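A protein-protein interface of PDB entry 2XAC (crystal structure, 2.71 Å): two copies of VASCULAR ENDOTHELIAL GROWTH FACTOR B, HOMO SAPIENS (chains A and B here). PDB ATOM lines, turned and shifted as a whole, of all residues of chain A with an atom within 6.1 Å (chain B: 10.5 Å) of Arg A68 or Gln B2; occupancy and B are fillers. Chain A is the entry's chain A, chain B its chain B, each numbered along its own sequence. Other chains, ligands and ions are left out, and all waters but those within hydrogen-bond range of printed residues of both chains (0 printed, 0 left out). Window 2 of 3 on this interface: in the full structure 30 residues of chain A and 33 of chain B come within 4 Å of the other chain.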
ATOM      1  N   HIS A  65      33.642 -25.904 -22.156  1.00  0.00           N
ATOM      2  CA  HIS A  65      32.776 -27.080 -22.107  1.00  0.00           C
ATOM      3  C   HIS A  65      32.281 -27.410 -23.511  1.00  0.00           C
ATOM      4  O   HIS A  65      32.362 -26.573 -24.414  1.00  0.00           O
ATOM      5  CB  HIS A  65      31.565 -26.810 -21.199  1.00  0.00           C
ATOM      6  CG  HIS A  65      30.724 -25.660 -21.656  1.00  0.00           C
ATOM      7  ND1 HIS A  65      30.972 -24.360 -21.272  1.00  0.00           N
ATOM      8  CD2 HIS A  65      29.665 -25.609 -22.498  1.00  0.00           C
ATOM      9  CE1 HIS A  65      30.093 -23.559 -21.849  1.00  0.00           C
ATOM     10  NE2 HIS A  65      29.290 -24.291 -22.598  1.00  0.00           N
ATOM     11  N   GLN A  66      31.751 -28.620 -23.683  1.00  0.00           N
ATOM     12  CA  GLN A  66      31.094 -29.006 -24.929  1.00  0.00           C
ATOM     13  C   GLN A  66      29.593 -28.758 -24.813  1.00  0.00           C
ATOM     14  O   GLN A  66      28.953 -29.204 -23.857  1.00  0.00           O
ATOM     15  CB  GLN A  66      31.350 -30.476 -25.261  1.00  0.00           C
ATOM     16  CG  GLN A  66      32.815 -30.855 -25.455  1.00  0.00           C
ATOM     17  CD  GLN A  66      33.414 -30.301 -26.735  1.00  0.00           C
ATOM     18  OE1 GLN A  66      34.143 -29.311 -26.709  1.00  0.00           O
ATOM     19  NE2 GLN A  66      33.106 -30.935 -27.863  1.00  0.00           N
ATOM     20  N   VAL A  67      29.039 -28.038 -25.785  1.00  0.00           N
ATOM     21  CA  VAL A  67      27.601 -27.804 -25.840  1.00  0.00           C
ATOM     22  C   VAL A  67      26.982 -28.887 -26.694  1.00  0.00           C
ATOM     23  O   VAL A  67      27.370 -29.066 -27.851  1.00  0.00           O
ATOM     24  CB  VAL A  67      27.226 -26.463 -26.516  1.00  0.00           C
ATOM     25  CG1 VAL A  67      26.286 -25.659 -25.627  1.00  0.00           C
ATOM     26  CG2 VAL A  67      28.454 -25.656 -26.864  1.00  0.00           C
ATOM     27  N   ARG A  68      26.026 -29.615 -26.127  1.00  0.00           N
ATOM     28  CA  ARG A  68      25.173 -30.468 -26.934  1.00  0.00           C
ATOM     29  C   ARG A  68      24.027 -29.588 -27.404  1.00  0.00           C
ATOM     30  O   ARG A  68      23.308 -28.992 -26.599  1.00  0.00           O
ATOM     31  CB  ARG A  68      24.638 -31.664 -26.147  1.00  0.00           C
ATOM     32  CG  ARG A  68      25.669 -32.440 -25.330  1.00  0.00           C
ATOM     33  CD  ARG A  68      25.426 -32.285 -23.825  1.00  0.00           C
ATOM     34  NE  ARG A  68      24.140 -32.845 -23.401  1.00  0.00           N
ATOM     35  CZ  ARG A  68      23.886 -34.146 -23.242  1.00  0.00           C
ATOM     36  NH1 ARG A  68      24.828 -35.058 -23.466  1.00  0.00           N
ATOM     37  NH2 ARG A  68      22.679 -34.541 -22.858  1.00  0.00           N
ATOM     38  N   MET A  69      23.892 -29.471 -28.716  1.00  0.00           N
ATOM     39  CA  MET A  69      22.760 -28.771 -29.302  1.00  0.00           C
ATOM     40  C   MET A  69      22.195 -29.595 -30.446  1.00  0.00           C
ATOM     41  O   MET A  69      22.933 -30.083 -31.301  1.00  0.00           O
ATOM     42  CB  MET A  69      23.133 -27.350 -29.747  1.00  0.00           C
ATOM     43  CG  MET A  69      24.440 -27.234 -30.512  1.00  0.00           C
ATOM     44  SD  MET A  69      24.930 -25.524 -30.821  1.00  0.00           S
ATOM     45  CE  MET A  69      24.792 -24.775 -29.200  1.00  0.00           C
ATOM     46  N   GLN A  70      20.878 -29.754 -30.434  1.00  0.00           N
ATOM     47  CA  GLN A  70      20.189 -30.556 -31.426  1.00  0.00           C
ATOM     48  C   GLN A  70      20.014 -29.830 -32.757  1.00  0.00           C
ATOM     49  O   GLN A  70      19.589 -28.670 -32.807  1.00  0.00           O
ATOM     50  CB  GLN A  70      18.851 -31.064 -30.889  1.00  0.00           C
ATOM     51  CG  GLN A  70      18.145 -30.118 -29.932  1.00  0.00           C
ATOM     52  CD  GLN A  70      17.069 -30.809 -29.114  1.00  0.00           C
ATOM     53  OE1 GLN A  70      17.222 -31.960 -28.704  1.00  0.00           O
ATOM     54  NE2 GLN A  70      15.975 -30.109 -28.873  1.00  0.00           N
ATOM     55  N   GLU A  83      22.010 -34.822 -32.134  1.00  0.00           N
ATOM     56  CA  GLU A  83      22.773 -34.032 -31.183  1.00  0.00           C
ATOM     57  C   GLU A  83      24.146 -33.662 -31.726  1.00  0.00           C
ATOM     58  O   GLU A  83      24.938 -34.535 -32.109  1.00  0.00           O
ATOM     59  CB  GLU A  83      22.902 -34.797 -29.873  1.00  0.00           C
ATOM     60  CG  GLU A  83      23.211 -33.931 -28.686  1.00  0.00           C
ATOM     61  CD  GLU A  83      22.651 -34.495 -27.400  1.00  0.00           C
ATOM     62  OE1 GLU A  83      23.457 -34.884 -26.526  1.00  0.00           O
ATOM     63  OE2 GLU A  83      21.409 -34.554 -27.265  1.00  0.00           O
ATOM     64  N   MET A  84      24.415 -32.358 -31.759  1.00  0.00           N
ATOM     65  CA  MET A  84      25.732 -31.836 -32.134  1.00  0.00           C
ATOM     66  C   MET A  84      26.479 -31.267 -30.937  1.00  0.00           C
ATOM     67  O   MET A  84      25.987 -30.377 -30.240  1.00  0.00           O
ATOM     68  CB  MET A  84      25.647 -30.773 -33.241  1.00  0.00           C
ATOM     69  CG  MET A  84      26.998 -30.103 -33.493  1.00  0.00           C
ATOM     70  SD  MET A  84      27.290 -29.461 -35.147  1.00  0.00           S
ATOM     71  CE  MET A  84      26.203 -28.046 -35.154  1.00  0.00           C
ATOM     72  N   SER A  85      27.681 -31.784 -30.723  1.00  0.00           N
ATOM     73  CA  SER A  85      28.545 -31.304 -29.664  1.00  0.00           C
ATOM     74  C   SER A  85      29.802 -30.683 -30.240  1.00  0.00           C
ATOM     75  O   SER A  85      30.387 -31.208 -31.186  1.00  0.00           O
ATOM     76  CB  SER A  85      28.884 -32.441 -28.712  1.00  0.00           C
ATOM     77  OG  SER A  85      27.743 -32.802 -27.956  1.00  0.00           O
ATOM     78  N   LEU A  86      30.188 -29.548 -29.665  1.00  0.00           N
ATOM     79  CA  LEU A  86      31.396 -28.808 -30.051  1.00  0.00           C
ATOM     80  C   LEU A  86      32.016 -28.035 -28.879  1.00  0.00           C
ATOM     81  O   LEU A  86      31.459 -28.004 -27.782  1.00  0.00           O
ATOM     82  CB  LEU A  86      31.112 -27.858 -31.226  1.00  0.00           C
ATOM     83  CG  LEU A  86      29.741 -27.219 -31.505  1.00  0.00           C
ATOM     84  CD1 LEU A  86      28.976 -26.773 -30.260  1.00  0.00           C
ATOM     85  CD2 LEU A  86      29.923 -26.050 -32.465  1.00  0.00           C
ATOM     86  N   GLN B   2      29.406 -29.518 -19.572  1.00  0.00           N
ATOM     87  CA  GLN B   2      28.334 -29.427 -20.608  1.00  0.00           C
ATOM     88  C   GLN B   2      27.143 -28.594 -20.128  1.00  0.00           C
ATOM     89  O   GLN B   2      27.056 -27.395 -20.413  1.00  0.00           O
ATOM     90  CB  GLN B   2      27.853 -30.827 -21.028  1.00  0.00           C
ATOM     91  CG  GLN B   2      28.904 -31.697 -21.714  1.00  0.00           C
ATOM     92  CD  GLN B   2      28.332 -32.982 -22.318  1.00  0.00           C
ATOM     93  OE1 GLN B   2      27.529 -33.681 -21.694  1.00  0.00           O
ATOM     94  NE2 GLN B   2      28.752 -33.297 -23.542  1.00  0.00           N
ATOM     95  N   ARG B   3      26.242 -29.246 -19.388  1.00  0.00           N
ATOM     96  CA  ARG B   3      24.967 -28.660 -18.971  1.00  0.00           C
ATOM     97  C   ARG B   3      23.802 -29.387 -19.624  1.00  0.00           C
ATOM     98  O   ARG B   3      23.726 -30.619 -19.584  1.00  0.00           O
ATOM     99  N   LYS B   4      22.902 -28.621 -20.238  1.00  0.00           N
ATOM    100  CA  LYS B   4      21.703 -29.172 -20.868  1.00  0.00           C
ATOM    101  C   LYS B   4      21.766 -29.018 -22.388  1.00  0.00           C
ATOM    102  O   LYS B   4      22.411 -28.097 -22.899  1.00  0.00           O
ATOM    103  CB  LYS B   4      20.432 -28.495 -20.317  1.00  0.00           C
ATOM    104  CG  LYS B   4      20.432 -28.216 -18.807  1.00  0.00           C
ATOM    105  CD  LYS B   4      20.643 -29.486 -17.971  1.00  0.00           C
ATOM    106  CE  LYS B   4      21.336 -29.168 -16.648  1.00  0.00           C
ATOM    107  NZ  LYS B   4      22.033 -30.357 -16.074  1.00  0.00           N
ATOM    108  N   VAL B   5      21.093 -29.922 -23.102  1.00  0.00           N
ATOM    109  CA  VAL B   5      21.039 -29.877 -24.560  1.00  0.00           C
ATOM    110  C   VAL B   5      20.241 -28.654 -24.994  1.00  0.00           C
ATOM    111  O   VAL B   5      19.042 -28.550 -24.700  1.00  0.00           O
ATOM    112  CB  VAL B   5      20.383 -31.149 -25.169  1.00  0.00           C
ATOM    113  CG1 VAL B   5      20.613 -31.212 -26.674  1.00  0.00           C
ATOM    114  CG2 VAL B   5      20.917 -32.410 -24.514  1.00  0.00           C
ATOM    115  N   VAL B   6      20.906 -27.726 -25.684  1.00  0.00           N
ATOM    116  CA  VAL B   6      20.237 -26.528 -26.197  1.00  0.00           C
ATOM    117  C   VAL B   6      19.196 -26.964 -27.211  1.00  0.00           C
ATOM    118  O   VAL B   6      19.526 -27.601 -28.210  1.00  0.00           O
ATOM    119  CB  VAL B   6      21.219 -25.521 -26.830  1.00  0.00           C
ATOM    120  CG1 VAL B   6      20.462 -24.366 -27.470  1.00  0.00           C
ATOM    121  CG2 VAL B   6      22.195 -24.995 -25.782  1.00  0.00           C
ATOM    122  N   SER B   7      17.938 -26.640 -26.926  1.00  0.00           N
ATOM    123  CA  SER B   7      16.811 -27.122 -27.716  1.00  0.00           C
ATOM    124  C   SER B   7      16.870 -26.587 -29.129  1.00  0.00           C
ATOM    125  O   SER B   7      17.325 -25.464 -29.343  1.00  0.00           O
ATOM    126  CB  SER B   7      15.507 -26.706 -27.063  1.00  0.00           C
ATOM    127  OG  SER B   7      14.454 -27.527 -27.529  1.00  0.00           O
ATOM    128  N   TRP B   8      16.403 -27.378 -30.091  1.00  0.00           N
ATOM    129  CA  TRP B   8      16.525 -27.006 -31.496  1.00  0.00           C
ATOM    130  C   TRP B   8      16.023 -25.599 -31.794  1.00  0.00           C
ATOM    131  O   TRP B   8      16.728 -24.812 -32.430  1.00  0.00           O
ATOM    132  CB  TRP B   8      15.834 -27.994 -32.425  1.00  0.00           C
ATOM    133  CG  TRP B   8      16.020 -27.585 -33.860  1.00  0.00           C
ATOM    134  CD1 TRP B   8      17.135 -27.780 -34.627  1.00  0.00           C
ATOM    135  CD2 TRP B   8      15.088 -26.874 -34.681  1.00  0.00           C
ATOM    136  NE1 TRP B   8      16.947 -27.247 -35.879  1.00  0.00           N
ATOM    137  CE2 TRP B   8      15.700 -26.685 -35.941  1.00  0.00           C
ATOM    138  CE3 TRP B   8      13.789 -26.384 -34.478  1.00  0.00           C
ATOM    139  CZ2 TRP B   8      15.058 -26.030 -36.998  1.00  0.00           C
ATOM    140  CZ3 TRP B   8      13.149 -25.730 -35.533  1.00  0.00           C
ATOM    141  CH2 TRP B   8      13.788 -25.560 -36.775  1.00  0.00           C
ATOM    142  N   ILE B   9      14.805 -25.302 -31.344  1.00  0.00           N
ATOM    143  CA  ILE B   9      14.225 -23.964 -31.438  1.00  0.00           C
ATOM    144  C   ILE B   9      15.254 -22.875 -31.180  1.00  0.00           C
ATOM    145  O   ILE B   9      15.345 -21.918 -31.941  1.00  0.00           O
ATOM    146  CB  ILE B   9      13.034 -23.776 -30.461  1.00  0.00           C
ATOM    147  CG1 ILE B   9      13.261 -24.572 -29.168  1.00  0.00           C
ATOM    148  CG2 ILE B   9      11.727 -24.192 -31.129  1.00  0.00           C
ATOM    149  CD1 ILE B   9      12.381 -24.146 -28.005  1.00  0.00           C
ATOM    150  N   ASP B  10      16.038 -23.034 -30.117  1.00  0.00           N
ATOM    151  CA  ASP B  10      17.007 -22.019 -29.718  1.00  0.00           C
ATOM    152  C   ASP B  10      18.264 -22.092 -30.553  1.00  0.00           C
ATOM    153  O   ASP B  10      18.886 -21.067 -30.834  1.00  0.00           O
ATOM    154  CB  ASP B  10      17.350 -22.154 -28.240  1.00  0.00           C
ATOM    155  CG  ASP B  10      16.131 -22.108 -27.361  1.00  0.00           C
ATOM    156  OD1 ASP B  10      16.076 -22.909 -26.409  1.00  0.00           O
ATOM    157  OD2 ASP B  10      15.222 -21.290 -27.629  1.00  0.00           O
ATOM    158  N   VAL B  11      18.642 -23.308 -30.941  1.00  0.00           N
ATOM    159  CA  VAL B  11      19.769 -23.489 -31.841  1.00  0.00           C
ATOM    160  C   VAL B  11      19.448 -22.715 -33.113  1.00  0.00           C
ATOM    161  O   VAL B  11      20.274 -21.936 -33.593  1.00  0.00           O
ATOM    162  CB  VAL B  11      20.038 -24.971 -32.172  1.00  0.00           C
ATOM    163  CG1 VAL B  11      21.328 -25.108 -32.974  1.00  0.00           C
ATOM    164  CG2 VAL B  11      20.125 -25.799 -30.907  1.00  0.00           C
ATOM    165  N   ARG B  14      19.067 -18.825 -32.287  1.00  0.00           N
ATOM    166  CA  ARG B  14      20.434 -18.314 -32.191  1.00  0.00           C
ATOM    167  C   ARG B  14      21.327 -18.851 -33.327  1.00  0.00           C
ATOM    168  O   ARG B  14      22.429 -19.355 -33.076  1.00  0.00           O
ATOM    169  CB  ARG B  14      21.026 -18.663 -30.820  1.00  0.00           C
ATOM    170  CG  ARG B  14      20.064 -18.479 -29.649  1.00  0.00           C
ATOM    171  CD  ARG B  14      20.496 -19.303 -28.440  1.00  0.00           C
ATOM    172  NE  ARG B  14      19.547 -19.221 -27.325  1.00  0.00           N
ATOM    173  CZ  ARG B  14      19.653 -19.914 -26.188  1.00  0.00           C
ATOM    174  NH1 ARG B  14      20.669 -20.755 -25.998  1.00  0.00           N
ATOM    175  NH2 ARG B  14      18.739 -19.770 -25.232  1.00  0.00           N
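NE2 of Gln A70 is in hydrogen-bond range of OG of Ser B7. The side-chain amide nitrogen of Gln A70 lies close to the backbone NH of Trp B8, at 3.0 Å. The backbone NH (N) of Gln A70 sits close to the backbone carbonyl oxygen (O) of Val B6. O of Arg A68 sits at hydrogen-bond distance from N of Val B6 (2.9 Å).
No position is printed for both chains.
Of the 11 printed residues of chain B, 7 touch a printed residue of chain A. Hydrophobic or aromatic side chains of chain B that line the printed part of chain A: Val B5, Val B6, Trp B8 and Val B11. Hydrophobic or aromatic side chains of chain A within 4 Å of the printed part of chain B: His A65 and Met A69. Among the printed residues, no Asp or Glu carboxylate lies within 4 Å of a Lys or Arg side-chain nitrogen of the other chain.
O of Leu A86 sits close to OE1 of Gln A66, at 3.2 Å. The guanidinium group (NH1) of Arg A68 is in salt-bridge range of the side-chain carboxylate (OE1) of Glu A83 (3.4 Å). O of Met A84 lies within hydrogen-bond range of N of Met A69, 2.7 Å away.
Among the printed residues, pairs that only touch across the chains: Arg A68 with Val B5 (3.2 Å), Gln A66 with Gln B2 (3.3 Å), Arg A68 with Gln B2 (3.3 Å), Gln A70 with Val B11 (3.5 Å), Glu A83 with Val B5 (3.5 Å), Met A69 with Val B11 (3.6 Å), Met A69 with Val B6 (3.6 Å), His A65 with Gln B2 (3.8 Å) and Arg A68 with Lys B4 (3.9 Å).
Gln B2 touches just these residues of chain A: His A65, Gln A66 and Arg A68. His A65 touches one residue of chain B. No residue of chain B comes within 4 Å of Val A67. Of chain B, only Val B6 (3.6 Å) and Val B11 (3.6 Å) come within 4 Å of Met A69. Of the printed residues of chain A, Trp B8 touches Gln A70 (3.0 Å). Printed residues of chain B within 4 Å of Gln A70: Val B6 (3.3 Å), Ser B7 (3.3 Å), Trp B8 (3.0 Å) and Val B11 (3.5 Å). Printed residues of chain A within 4 Å of Val B11: Met A69 and Gln A70. Of the printed residues of chain A, Val B5 touches Arg A68 and Glu A83. Printed residues of chain B within 4 Å of Glu A83: Val B5 (3.5 Å). Asp B10 touches none of the printed residues of chain A. Leu A86 touches none of the printed residues of chain B. The nearest residue of chain B that does not touch Arg A68 is Arg B3 (4.4 Å). The nearest residue of chain A that does not touch Gln B2 is Ser A85 (4.6 Å).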
